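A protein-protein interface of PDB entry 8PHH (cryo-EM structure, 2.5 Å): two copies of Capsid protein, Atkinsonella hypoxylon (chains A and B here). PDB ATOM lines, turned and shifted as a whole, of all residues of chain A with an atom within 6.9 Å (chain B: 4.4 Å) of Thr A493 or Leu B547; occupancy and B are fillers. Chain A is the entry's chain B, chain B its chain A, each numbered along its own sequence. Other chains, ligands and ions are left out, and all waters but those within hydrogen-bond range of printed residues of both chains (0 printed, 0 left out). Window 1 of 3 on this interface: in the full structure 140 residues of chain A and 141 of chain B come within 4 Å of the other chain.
The backbone carbonyl oxygen (O) of Asn A488 sits at hydrogen-bond distance from the backbone NH (N) of Phe B549, 3.1 Å away.
The backbone carbonyl oxygen (O) of Leu B547 is in hydrogen-bond range of the backbone NH (N) of Asp A490 (2.9 Å).
The backbone carbonyl oxygen (O) of Gly A491 sits at hydrogen-bond distance from the backbone NH (N) of Leu B547 (2.8 Å).
OE2 of Glu A492 is in hydrogen-bond range of OG1 of Thr B546 (3.0 Å).
The side-chain hydroxyl (OG1) of Thr A493 is in hydrogen-bond range of the side-chain hydroxyl (OG1) of Thr B493 (2.9 Å).
O of Leu B545 lies within hydrogen-bond range of N of Thr A493 (2.9 Å).
The backbone NH (N) of Leu A494 sits at hydrogen-bond distance from the backbone carbonyl oxygen (O) of Glu B492.
The backbone carbonyl oxygen of Leu A545 lies within hydrogen-bond range of the backbone NH of Thr B493 (3.1 Å).
The backbone carbonyl oxygen of Gly B491 sits at hydrogen-bond distance from the backbone NH of Leu A547.
The backbone NH of Leu B548 sits at hydrogen-bond distance from the backbone carbonyl oxygen of Asn A586, at 2.8 Å.
The backbone carbonyl oxygen (O) of Thr B546 lies within hydrogen-bond range of the backbone NH (N) of Val A588, at 3.2 Å.
The backbone carbonyl oxygen (O) of Thr A493 lies close to the side-chain amide oxygen (OE1) of Gln A512 (3.0 Å).
The backbone NH of Leu A495 is in hydrogen-bond range of the side-chain amide oxygen of Gln A512 (3.3 Å).
N of Leu A495 sits close to SD of Met A551.
Among the printed residues, merely in contact across the chains: Ile A489 with Thr B546 (3.3 Å), Leu A494 with Gly B491 (3.3 Å), Asp A490 with Asn B550 (3.3 Å), Val A588 with Leu B545 (3.3 Å), Asn A586 with Leu B547 (3.3 Å), Glu A492 with Thr B493 (3.4 Å), Thr A493 with Glu B492 (3.4 Å), Met A551 with Leu B545 (3.4 Å), Gly A491 with Thr B546 (3.4 Å), Asn A586 with Asn B550 (3.5 Å), Asp A490 with Met B551 (3.6 Å), Leu A545 with Met B551 (3.6 Å), Asn A488 with Leu B548 (3.6 Å), Val A554 with Val B554 (3.6 Å), Glu A492 with Leu B545 (3.7 Å), Thr A493 with Ser B544 (3.7 Å), Gly A513 with Ser B544 (3.7 Å), Leu A545 with Leu B547 (3.7 Å), Leu A547 with Leu B545 (3.7 Å), Ile A489 with Leu B547 (3.7 Å), Leu A545 with Glu B492 (3.7 Å), Val A587 with Leu B545 (3.7 Å), Asp A490 with Phe B549 (3.7 Å), Asn A586 with Val B554 (3.7 Å), Val A587 with Val B554 (3.7 Å), Met A551 with Ser B544 (3.8 Å), Ile A489 with Leu B548 (3.8 Å), Asn A586 with Thr B546 (3.8 Å), Thr A493 with Gly B491 (3.8 Å), Val A588 with Leu B548 (3.8 Å), Glu A492 with Ser B544 (3.9 Å), Val A587 with Thr B546 (3.9 Å), Leu A511 with Ser B544 (3.9 Å), Thr A493 with Leu B547 (3.9 Å), Glu A492 with Glu B492 (3.9 Å), Gly A491 with Thr B493 (3.98 Å) and Gln A512 with Ser B544 (3.99 Å).
Of chain B, only Gly B491, Glu B492, Thr B493, Ser B544, Leu B545 and Leu B547 come within 4 Å of Thr A493.
Leu B547 touches just these residues of chain A: Ile A489, Asp A490, Gly A491, Thr A493, Leu A545 and Asn A586.
Of the printed residues of chain B, Met A551 touches Ser B544 and Leu B545.
Printed residues of chain A within 4 Å of Ser B544: Glu A492, Thr A493, Leu A511, Gln A512, Gly A513 and Met A551.
Of the printed residues of chain B, Glu A492 touches Glu B492 (3.9 Å), Thr B493 (3.4 Å), Ser B544 (3.9 Å), Leu B545 (3.7 Å) and Thr B546 (3.0 Å).
Printed residues of chain A within 4 Å of Thr B493: Gly A491 (3.98 Å), Glu A492 (3.4 Å), Thr A493 (2.9 Å) and Leu A545 (3.1 Å).
Leu A495 touches none of the printed residues of chain B.
Leu A631 touches none of the printed residues of chain B.
The nearest printed residue of chain B that does not touch Val A554 is Leu B545 (4.02 Å).
Hydrophobic or aromatic side chains of chain A within 4 Å of the printed part of chain B: Ile A489, Leu A494, Leu A545, Leu A547, Met A551, Val A554, Val A587 and Val A588.
Printed residues of chain B that touch a printed residue of chain A: Gly B491, Glu B492, Thr B493, Ser B544, Leu B545, Thr B546, Leu B547, Leu B548, Phe B549, Asn B550, Met B551 and Val B554.
Hydrophobic or aromatic side chains of chain B within 4 Å of the printed part of chain A: Leu B545, Leu B547, Leu B548, Phe B549 and Val B554.
Along chain B the printed residues that touch a printed residue of chain A span positions 491 to 554.
Among the printed residues, 48 pairs touch across the chains.
Among the printed residues, no Asp or Glu carboxylate lies within 4 Å of a Lys or Arg side-chain nitrogen of the other chain.
Gly A491 touches Thr B493, and with the chains exchanged Thr A493 touches Gly B491.
Glu A492 touches its own counterpart, Glu B492.
Glu A492 touches Thr B493, and with the chains exchanged Thr A493 touches Glu B492.
Glu A492 touches Leu B545, and with the chains exchanged Leu A545 touches Glu B492.
Of the 48 pairs that touch across the chains among the printed residues, 17 have their exchanged pair printed and touching as well.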
ATOM      1  N   ASN A 488     -12.075   9.028 -36.212  1.00  0.00           N
ATOM      2  CA  ASN A 488     -11.947   7.610 -36.522  1.00  0.00           C
ATOM      3  C   ASN A 488     -11.949   6.670 -35.317  1.00  0.00           C
ATOM      4  O   ASN A 488     -11.837   5.458 -35.510  1.00  0.00           O
ATOM      5  CB  ASN A 488     -10.691   7.354 -37.370  1.00  0.00           C
ATOM      6  CG  ASN A 488      -9.407   7.787 -36.694  1.00  0.00           C
ATOM      7  OD1 ASN A 488      -9.405   8.305 -35.580  1.00  0.00           O
ATOM      8  ND2 ASN A 488      -8.293   7.543 -37.361  1.00  0.00           N
ATOM      9  N   ILE A 489     -12.073   7.165 -34.095  1.00  0.00           N
ATOM     10  CA  ILE A 489     -12.088   6.267 -32.946  1.00  0.00           C
ATOM     11  C   ILE A 489     -13.491   5.707 -32.779  1.00  0.00           C
ATOM     12  O   ILE A 489     -14.470   6.461 -32.724  1.00  0.00           O
ATOM     13  CB  ILE A 489     -11.633   6.986 -31.670  1.00  0.00           C
ATOM     14  CG1 ILE A 489     -10.258   7.608 -31.848  1.00  0.00           C
ATOM     15  CG2 ILE A 489     -11.541   6.015 -30.545  1.00  0.00           C
ATOM     16  CD1 ILE A 489      -9.925   8.555 -30.744  1.00  0.00           C
ATOM     17  N   ASP A 490     -13.597   4.385 -32.698  1.00  0.00           N
ATOM     18  CA  ASP A 490     -14.887   3.726 -32.554  1.00  0.00           C
ATOM     19  C   ASP A 490     -15.098   3.119 -31.176  1.00  0.00           C
ATOM     20  O   ASP A 490     -16.234   2.846 -30.797  1.00  0.00           O
ATOM     21  CB  ASP A 490     -15.039   2.634 -33.620  1.00  0.00           C
ATOM     22  CG  ASP A 490     -16.487   2.326 -33.940  1.00  0.00           C
ATOM     23  OD1 ASP A 490     -17.386   2.988 -33.387  1.00  0.00           O
ATOM     24  OD2 ASP A 490     -16.736   1.426 -34.759  1.00  0.00           O
ATOM     25  N   GLY A 491     -14.046   2.920 -30.399  1.00  0.00           N
ATOM     26  CA  GLY A 491     -14.191   2.259 -29.116  1.00  0.00           C
ATOM     27  C   GLY A 491     -13.123   2.653 -28.126  1.00  0.00           C
ATOM     28  O   GLY A 491     -11.973   2.910 -28.490  1.00  0.00           O
ATOM     29  N   GLU A 492     -13.514   2.689 -26.859  1.00  0.00           N
ATOM     30  CA  GLU A 492     -12.621   2.910 -25.734  1.00  0.00           C
ATOM     31  C   GLU A 492     -12.904   1.846 -24.686  1.00  0.00           C
ATOM     32  O   GLU A 492     -14.065   1.572 -24.373  1.00  0.00           O
ATOM     33  CB  GLU A 492     -12.817   4.298 -25.118  1.00  0.00           C
ATOM     34  CG  GLU A 492     -12.458   5.473 -26.015  1.00  0.00           C
ATOM     35  CD  GLU A 492     -10.971   5.605 -26.274  1.00  0.00           C
ATOM     36  OE1 GLU A 492     -10.173   5.204 -25.405  1.00  0.00           O
ATOM     37  OE2 GLU A 492     -10.601   6.134 -27.339  1.00  0.00           O
ATOM     38  N   THR A 493     -11.851   1.256 -24.142  1.00  0.00           N
ATOM     39  CA  THR A 493     -11.979   0.180 -23.175  1.00  0.00           C
ATOM     40  C   THR A 493     -11.839   0.705 -21.750  1.00  0.00           C
ATOM     41  O   THR A 493     -10.912   1.451 -21.433  1.00  0.00           O
ATOM     42  CB  THR A 493     -10.934  -0.901 -23.446  1.00  0.00           C
ATOM     43  OG1 THR A 493     -11.093  -1.380 -24.784  1.00  0.00           O
ATOM     44  CG2 THR A 493     -11.102  -2.059 -22.494  1.00  0.00           C
ATOM     45  N   LEU A 494     -12.778   0.311 -20.896  1.00  0.00           N
ATOM     46  CA  LEU A 494     -12.769   0.638 -19.477  1.00  0.00           C
ATOM     47  C   LEU A 494     -12.032  -0.442 -18.702  1.00  0.00           C
ATOM     48  O   LEU A 494     -12.197  -1.630 -18.987  1.00  0.00           O
ATOM     49  CB  LEU A 494     -14.196   0.766 -18.950  1.00  0.00           C
ATOM     50  CG  LEU A 494     -14.399   1.143 -17.488  1.00  0.00           C
ATOM     51  CD1 LEU A 494     -13.866   2.527 -17.211  1.00  0.00           C
ATOM     52  CD2 LEU A 494     -15.862   1.058 -17.140  1.00  0.00           C
ATOM     53  N   LEU A 495     -11.224  -0.035 -17.730  1.00  0.00           N
ATOM     54  CA  LEU A 495     -10.629  -0.983 -16.800  1.00  0.00           C
ATOM     55  C   LEU A 495     -11.648  -1.344 -15.732  1.00  0.00           C
ATOM     56  O   LEU A 495     -12.205  -0.463 -15.074  1.00  0.00           O
ATOM     57  CB  LEU A 495      -9.375  -0.396 -16.160  1.00  0.00           C
ATOM     58  CG  LEU A 495      -8.551  -1.295 -15.239  1.00  0.00           C
ATOM     59  CD1 LEU A 495      -8.021  -2.481 -15.996  1.00  0.00           C
ATOM     60  CD2 LEU A 495      -7.423  -0.512 -14.627  1.00  0.00           C
ATOM     61  N   LEU A 511      -7.678   8.108 -16.514  1.00  0.00           N
ATOM     62  CA  LEU A 511      -7.236   8.226 -17.894  1.00  0.00           C
ATOM     63  C   LEU A 511      -7.946   7.267 -18.831  1.00  0.00           C
ATOM     64  O   LEU A 511      -7.480   7.064 -19.955  1.00  0.00           O
ATOM     65  CB  LEU A 511      -5.727   8.007 -17.993  1.00  0.00           C
ATOM     66  CG  LEU A 511      -4.814   9.092 -17.449  1.00  0.00           C
ATOM     67  CD1 LEU A 511      -3.376   8.649 -17.529  1.00  0.00           C
ATOM     68  CD2 LEU A 511      -5.015  10.366 -18.232  1.00  0.00           C
ATOM     69  N   GLN A 512      -9.053   6.673 -18.401  1.00  0.00           N
ATOM     70  CA  GLN A 512      -9.823   5.807 -19.277  1.00  0.00           C
ATOM     71  C   GLN A 512     -10.555   6.649 -20.311  1.00  0.00           C
ATOM     72  O   GLN A 512     -11.304   7.565 -19.965  1.00  0.00           O
ATOM     73  CB  GLN A 512     -10.818   4.984 -18.465  1.00  0.00           C
ATOM     74  CG  GLN A 512     -10.186   4.127 -17.397  1.00  0.00           C
ATOM     75  CD  GLN A 512      -9.267   3.075 -17.957  1.00  0.00           C
ATOM     76  OE1 GLN A 512      -9.550   2.468 -18.988  1.00  0.00           O
ATOM     77  NE2 GLN A 512      -8.150   2.855 -17.284  1.00  0.00           N
ATOM     78  N   GLY A 513     -10.341   6.335 -21.583  1.00  0.00           N
ATOM     79  CA  GLY A 513     -10.911   7.135 -22.643  1.00  0.00           C
ATOM     80  C   GLY A 513     -10.009   8.240 -23.122  1.00  0.00           C
ATOM     81  O   GLY A 513     -10.475   9.168 -23.786  1.00  0.00           O
ATOM     82  N   LEU A 545     -17.284  -5.659 -26.930  1.00  0.00           N
ATOM     83  CA  LEU A 545     -15.973  -6.285 -26.984  1.00  0.00           C
ATOM     84  C   LEU A 545     -15.493  -6.518 -25.564  1.00  0.00           C
ATOM     85  O   LEU A 545     -15.462  -5.583 -24.760  1.00  0.00           O
ATOM     86  CB  LEU A 545     -14.961  -5.421 -27.731  1.00  0.00           C
ATOM     87  CG  LEU A 545     -13.713  -6.229 -28.045  1.00  0.00           C
ATOM     88  CD1 LEU A 545     -14.077  -7.225 -29.114  1.00  0.00           C
ATOM     89  CD2 LEU A 545     -12.575  -5.371 -28.480  1.00  0.00           C
ATOM     90  N   LEU A 547     -12.412  -7.939 -23.116  1.00  0.00           N
ATOM     91  CA  LEU A 547     -10.988  -8.236 -23.015  1.00  0.00           C
ATOM     92  C   LEU A 547     -10.733  -9.075 -21.773  1.00  0.00           C
ATOM     93  O   LEU A 547     -11.172  -8.724 -20.675  1.00  0.00           O
ATOM     94  CB  LEU A 547     -10.162  -6.957 -22.985  1.00  0.00           C
ATOM     95  CG  LEU A 547     -10.081  -6.205 -24.300  1.00  0.00           C
ATOM     96  CD1 LEU A 547      -9.384  -4.910 -24.073  1.00  0.00           C
ATOM     97  CD2 LEU A 547      -9.318  -7.026 -25.303  1.00  0.00           C
ATOM     98  N   MET A 551      -6.214  -5.820 -20.348  1.00  0.00           N
ATOM     99  CA  MET A 551      -6.801  -4.950 -21.355  1.00  0.00           C
ATOM    100  C   MET A 551      -5.767  -4.098 -22.074  1.00  0.00           C
ATOM    101  O   MET A 551      -6.116  -3.423 -23.046  1.00  0.00           O
ATOM    102  CB  MET A 551      -7.843  -4.012 -20.755  1.00  0.00           C
ATOM    103  CG  MET A 551      -7.224  -2.867 -20.013  1.00  0.00           C
ATOM    104  SD  MET A 551      -8.362  -1.543 -19.660  1.00  0.00           S
ATOM    105  CE  MET A 551      -7.185  -0.347 -19.059  1.00  0.00           C
ATOM    106  N   VAL A 554      -3.689  -6.453 -27.077  1.00  0.00           N
ATOM    107  CA  VAL A 554      -4.420  -7.545 -27.699  1.00  0.00           C
ATOM    108  C   VAL A 554      -3.419  -8.589 -28.157  1.00  0.00           C
ATOM    109  O   VAL A 554      -2.536  -8.300 -28.969  1.00  0.00           O
ATOM    110  CB  VAL A 554      -5.278  -7.060 -28.871  1.00  0.00           C
ATOM    111  CG1 VAL A 554      -5.874  -8.255 -29.550  1.00  0.00           C
ATOM    112  CG2 VAL A 554      -6.370  -6.141 -28.378  1.00  0.00           C
ATOM    113  N   ASN A 586      -6.130  -2.052 -35.861  1.00  0.00           N
ATOM    114  CA  ASN A 586      -7.158  -1.154 -35.365  1.00  0.00           C
ATOM    115  C   ASN A 586      -6.984  -0.870 -33.881  1.00  0.00           C
ATOM    116  O   ASN A 586      -7.841  -0.256 -33.250  1.00  0.00           O
ATOM    117  CB  ASN A 586      -8.554  -1.703 -35.652  1.00  0.00           C
ATOM    118  CG  ASN A 586      -8.806  -3.068 -35.047  1.00  0.00           C
ATOM    119  OD1 ASN A 586      -7.928  -3.692 -34.453  1.00  0.00           O
ATOM    120  ND2 ASN A 586     -10.041  -3.526 -35.170  1.00  0.00           N
ATOM    121  N   VAL A 587      -5.870  -1.315 -33.319  1.00  0.00           N
ATOM    122  CA  VAL A 587      -5.633  -1.260 -31.888  1.00  0.00           C
ATOM    123  C   VAL A 587      -4.473  -0.319 -31.629  1.00  0.00           C
ATOM    124  O   VAL A 587      -3.391  -0.486 -32.200  1.00  0.00           O
ATOM    125  CB  VAL A 587      -5.348  -2.659 -31.313  1.00  0.00           C
ATOM    126  CG1 VAL A 587      -4.913  -2.572 -29.877  1.00  0.00           C
ATOM    127  CG2 VAL A 587      -6.585  -3.511 -31.410  1.00  0.00           C
ATOM    128  N   VAL A 588      -4.703   0.676 -30.783  1.00  0.00           N
ATOM    129  CA  VAL A 588      -3.666   1.579 -30.314  1.00  0.00           C
ATOM    130  C   VAL A 588      -3.471   1.315 -28.829  1.00  0.00           C
ATOM    131  O   VAL A 588      -4.383   1.539 -28.027  1.00  0.00           O
ATOM    132  CB  VAL A 588      -4.028   3.044 -30.583  1.00  0.00           C
ATOM    133  CG1 VAL A 588      -3.008   3.956 -29.958  1.00  0.00           C
ATOM    134  CG2 VAL A 588      -4.136   3.298 -32.067  1.00  0.00           C
ATOM    135  N   LEU A 631     -16.904   7.346 -20.010  1.00  0.00           N
ATOM    136  CA  LEU A 631     -16.360   6.415 -19.033  1.00  0.00           C
ATOM    137  C   LEU A 631     -16.417   7.023 -17.644  1.00  0.00           C
ATOM    138  O   LEU A 631     -16.597   6.310 -16.652  1.00  0.00           O
ATOM    139  CB  LEU A 631     -14.937   6.016 -19.405  1.00  0.00           C
ATOM    140  CG  LEU A 631     -14.868   5.248 -20.724  1.00  0.00           C
ATOM    141  CD1 LEU A 631     -13.463   4.887 -21.096  1.00  0.00           C
ATOM    142  CD2 LEU A 631     -15.701   4.017 -20.667  1.00  0.00           C
ATOM    143  N   GLY B 491     -11.377  -5.947 -19.155  1.00  0.00           N
ATOM    144  CA  GLY B 491     -11.783  -4.757 -19.881  1.00  0.00           C
ATOM    145  C   GLY B 491     -13.080  -4.929 -20.634  1.00  0.00           C
ATOM    146  O   GLY B 491     -13.371  -6.000 -21.174  1.00  0.00           O
ATOM    147  N   GLU B 492     -13.861  -3.851 -20.680  1.00  0.00           N
ATOM    148  CA  GLU B 492     -15.068  -3.753 -21.486  1.00  0.00           C
ATOM    149  C   GLU B 492     -15.001  -2.503 -22.352  1.00  0.00           C
ATOM    150  O   GLU B 492     -14.651  -1.422 -21.876  1.00  0.00           O
ATOM    151  CB  GLU B 492     -16.332  -3.698 -20.619  1.00  0.00           C
ATOM    152  CG  GLU B 492     -16.646  -4.965 -19.851  1.00  0.00           C
ATOM    153  CD  GLU B 492     -17.060  -6.119 -20.743  1.00  0.00           C
ATOM    154  OE1 GLU B 492     -17.660  -5.868 -21.809  1.00  0.00           O
ATOM    155  OE2 GLU B 492     -16.799  -7.280 -20.373  1.00  0.00           O
ATOM    156  N   THR B 493     -15.345  -2.651 -23.628  1.00  0.00           N
ATOM    157  CA  THR B 493     -15.179  -1.591 -24.614  1.00  0.00           C
ATOM    158  C   THR B 493     -16.508  -0.893 -24.864  1.00  0.00           C
ATOM    159  O   THR B 493     -17.525  -1.550 -25.103  1.00  0.00           O
ATOM    160  CB  THR B 493     -14.621  -2.146 -25.922  1.00  0.00           C
ATOM    161  OG1 THR B 493     -13.416  -2.865 -25.650  1.00  0.00           O
ATOM    162  CG2 THR B 493     -14.291  -1.028 -26.877  1.00  0.00           C
ATOM    163  N   SER B 544      -5.064   2.418 -20.836  1.00  0.00           N
ATOM    164  CA  SER B 544      -6.307   2.316 -21.582  1.00  0.00           C
ATOM    165  C   SER B 544      -6.050   1.612 -22.907  1.00  0.00           C
ATOM    166  O   SER B 544      -4.917   1.258 -23.241  1.00  0.00           O
ATOM    167  CB  SER B 544      -6.931   3.694 -21.831  1.00  0.00           C
ATOM    168  OG  SER B 544      -8.142   3.567 -22.560  1.00  0.00           O
ATOM    169  N   LEU B 545      -7.126   1.402 -23.661  1.00  0.00           N
ATOM    170  CA  LEU B 545      -7.043   0.795 -24.979  1.00  0.00           C
ATOM    171  C   LEU B 545      -8.111   1.403 -25.870  1.00  0.00           C
ATOM    172  O   LEU B 545      -9.287   1.437 -25.498  1.00  0.00           O
ATOM    173  CB  LEU B 545      -7.221  -0.720 -24.923  1.00  0.00           C
ATOM    174  CG  LEU B 545      -6.863  -1.403 -26.237  1.00  0.00           C
ATOM    175  CD1 LEU B 545      -5.383  -1.226 -26.472  1.00  0.00           C
ATOM    176  CD2 LEU B 545      -7.211  -2.855 -26.217  1.00  0.00           C
ATOM    177  N   THR B 546      -7.707   1.870 -27.043  1.00  0.00           N
ATOM    178  CA  THR B 546      -8.605   2.534 -27.973  1.00  0.00           C
ATOM    179  C   THR B 546      -8.653   1.772 -29.289  1.00  0.00           C
ATOM    180  O   THR B 546      -7.624   1.309 -29.788  1.00  0.00           O
ATOM    181  CB  THR B 546      -8.188   3.997 -28.171  1.00  0.00           C
ATOM    182  OG1 THR B 546      -8.913   4.576 -29.259  1.00  0.00           O
ATOM    183  CG2 THR B 546      -6.710   4.148 -28.370  1.00  0.00           C
ATOM    184  N   LEU B 547      -9.859   1.620 -29.829  1.00  0.00           N
ATOM    185  CA  LEU B 547     -10.088   0.847 -31.041  1.00  0.00           C
ATOM    186  C   LEU B 547     -10.529   1.769 -32.160  1.00  0.00           C
ATOM    187  O   LEU B 547     -11.402   2.620 -31.968  1.00  0.00           O
ATOM    188  CB  LEU B 547     -11.127  -0.252 -30.831  1.00  0.00           C
ATOM    189  CG  LEU B 547     -10.605  -1.522 -30.171  1.00  0.00           C
ATOM    190  CD1 LEU B 547     -10.647  -1.444 -28.654  1.00  0.00           C
ATOM    191  CD2 LEU B 547     -11.306  -2.734 -30.704  1.00  0.00           C
ATOM    192  N   LEU B 548      -9.935   1.581 -33.326  1.00  0.00           N
ATOM    193  CA  LEU B 548     -10.161   2.434 -34.474  1.00  0.00           C
ATOM    194  C   LEU B 548     -11.007   1.710 -35.511  1.00  0.00           C
ATOM    195  O   LEU B 548     -10.898   0.499 -35.700  1.00  0.00           O
ATOM    196  CB  LEU B 548      -8.830   2.849 -35.092  1.00  0.00           C
ATOM    197  CG  LEU B 548      -7.837   3.613 -34.225  1.00  0.00           C
ATOM    198  CD1 LEU B 548      -6.546   3.818 -34.982  1.00  0.00           C
ATOM    199  CD2 LEU B 548      -8.405   4.936 -33.768  1.00  0.00           C
ATOM    200  N   PHE B 549     -11.921   2.464 -36.118  1.00  0.00           N
ATOM    201  CA  PHE B 549     -12.714   2.178 -37.318  1.00  0.00           C
ATOM    202  C   PHE B 549     -13.782   1.103 -37.121  1.00  0.00           C
ATOM    203  O   PHE B 549     -14.765   1.075 -37.867  1.00  0.00           O
ATOM    204  CB  PHE B 549     -11.834   1.711 -38.493  1.00  0.00           C
ATOM    205  CG  PHE B 549     -10.580   2.500 -38.686  1.00  0.00           C
ATOM    206  CD1 PHE B 549     -10.614   3.813 -39.117  1.00  0.00           C
ATOM    207  CD2 PHE B 549      -9.353   1.895 -38.492  1.00  0.00           C
ATOM    208  CE1 PHE B 549      -9.441   4.517 -39.294  1.00  0.00           C
ATOM    209  CE2 PHE B 549      -8.185   2.592 -38.669  1.00  0.00           C
ATOM    210  CZ  PHE B 549      -8.227   3.900 -39.077  1.00  0.00           C
ATOM    211  N   ASN B 550     -13.632   0.267 -36.095  1.00  0.00           N
ATOM    212  CA  ASN B 550     -14.540  -0.829 -35.775  1.00  0.00           C
ATOM    213  C   ASN B 550     -14.108  -1.374 -34.427  1.00  0.00           C
ATOM    214  O   ASN B 550     -12.946  -1.754 -34.266  1.00  0.00           O
ATOM    215  CB  ASN B 550     -14.502  -1.937 -36.830  1.00  0.00           C
ATOM    216  CG  ASN B 550     -15.672  -2.877 -36.721  1.00  0.00           C
ATOM    217  OD1 ASN B 550     -16.530  -2.721 -35.856  1.00  0.00           O
ATOM    218  ND2 ASN B 550     -15.716  -3.863 -37.599  1.00  0.00           N
ATOM    219  N   MET B 551     -15.019  -1.435 -33.465  1.00  0.00           N
ATOM    220  CA  MET B 551     -14.661  -2.001 -32.175  1.00  0.00           C
ATOM    221  C   MET B 551     -15.123  -3.441 -32.029  1.00  0.00           C
ATOM    222  O   MET B 551     -14.747  -4.110 -31.063  1.00  0.00           O
ATOM    223  CB  MET B 551     -15.239  -1.175 -31.030  1.00  0.00           C
ATOM    224  CG  MET B 551     -16.671  -1.479 -30.727  1.00  0.00           C
ATOM    225  SD  MET B 551     -17.113  -0.722 -29.178  1.00  0.00           S
ATOM    226  CE  MET B 551     -18.614  -1.596 -28.820  1.00  0.00           C
ATOM    227  N   VAL B 554     -11.076  -7.324 -33.657  1.00  0.00           N
ATOM    228  CA  VAL B 554      -9.687  -6.888 -33.653  1.00  0.00           C
ATOM    229  C   VAL B 554      -9.024  -7.451 -34.899  1.00  0.00           C
ATOM    230  O   VAL B 554      -9.050  -8.663 -35.133  1.00  0.00           O
ATOM    231  CB  VAL B 554      -8.948  -7.333 -32.389  1.00  0.00           C
ATOM    232  CG1 VAL B 554      -7.492  -6.976 -32.520  1.00  0.00           C
ATOM    233  CG2 VAL B 554      -9.545  -6.663 -31.177  1.00  0.00           C
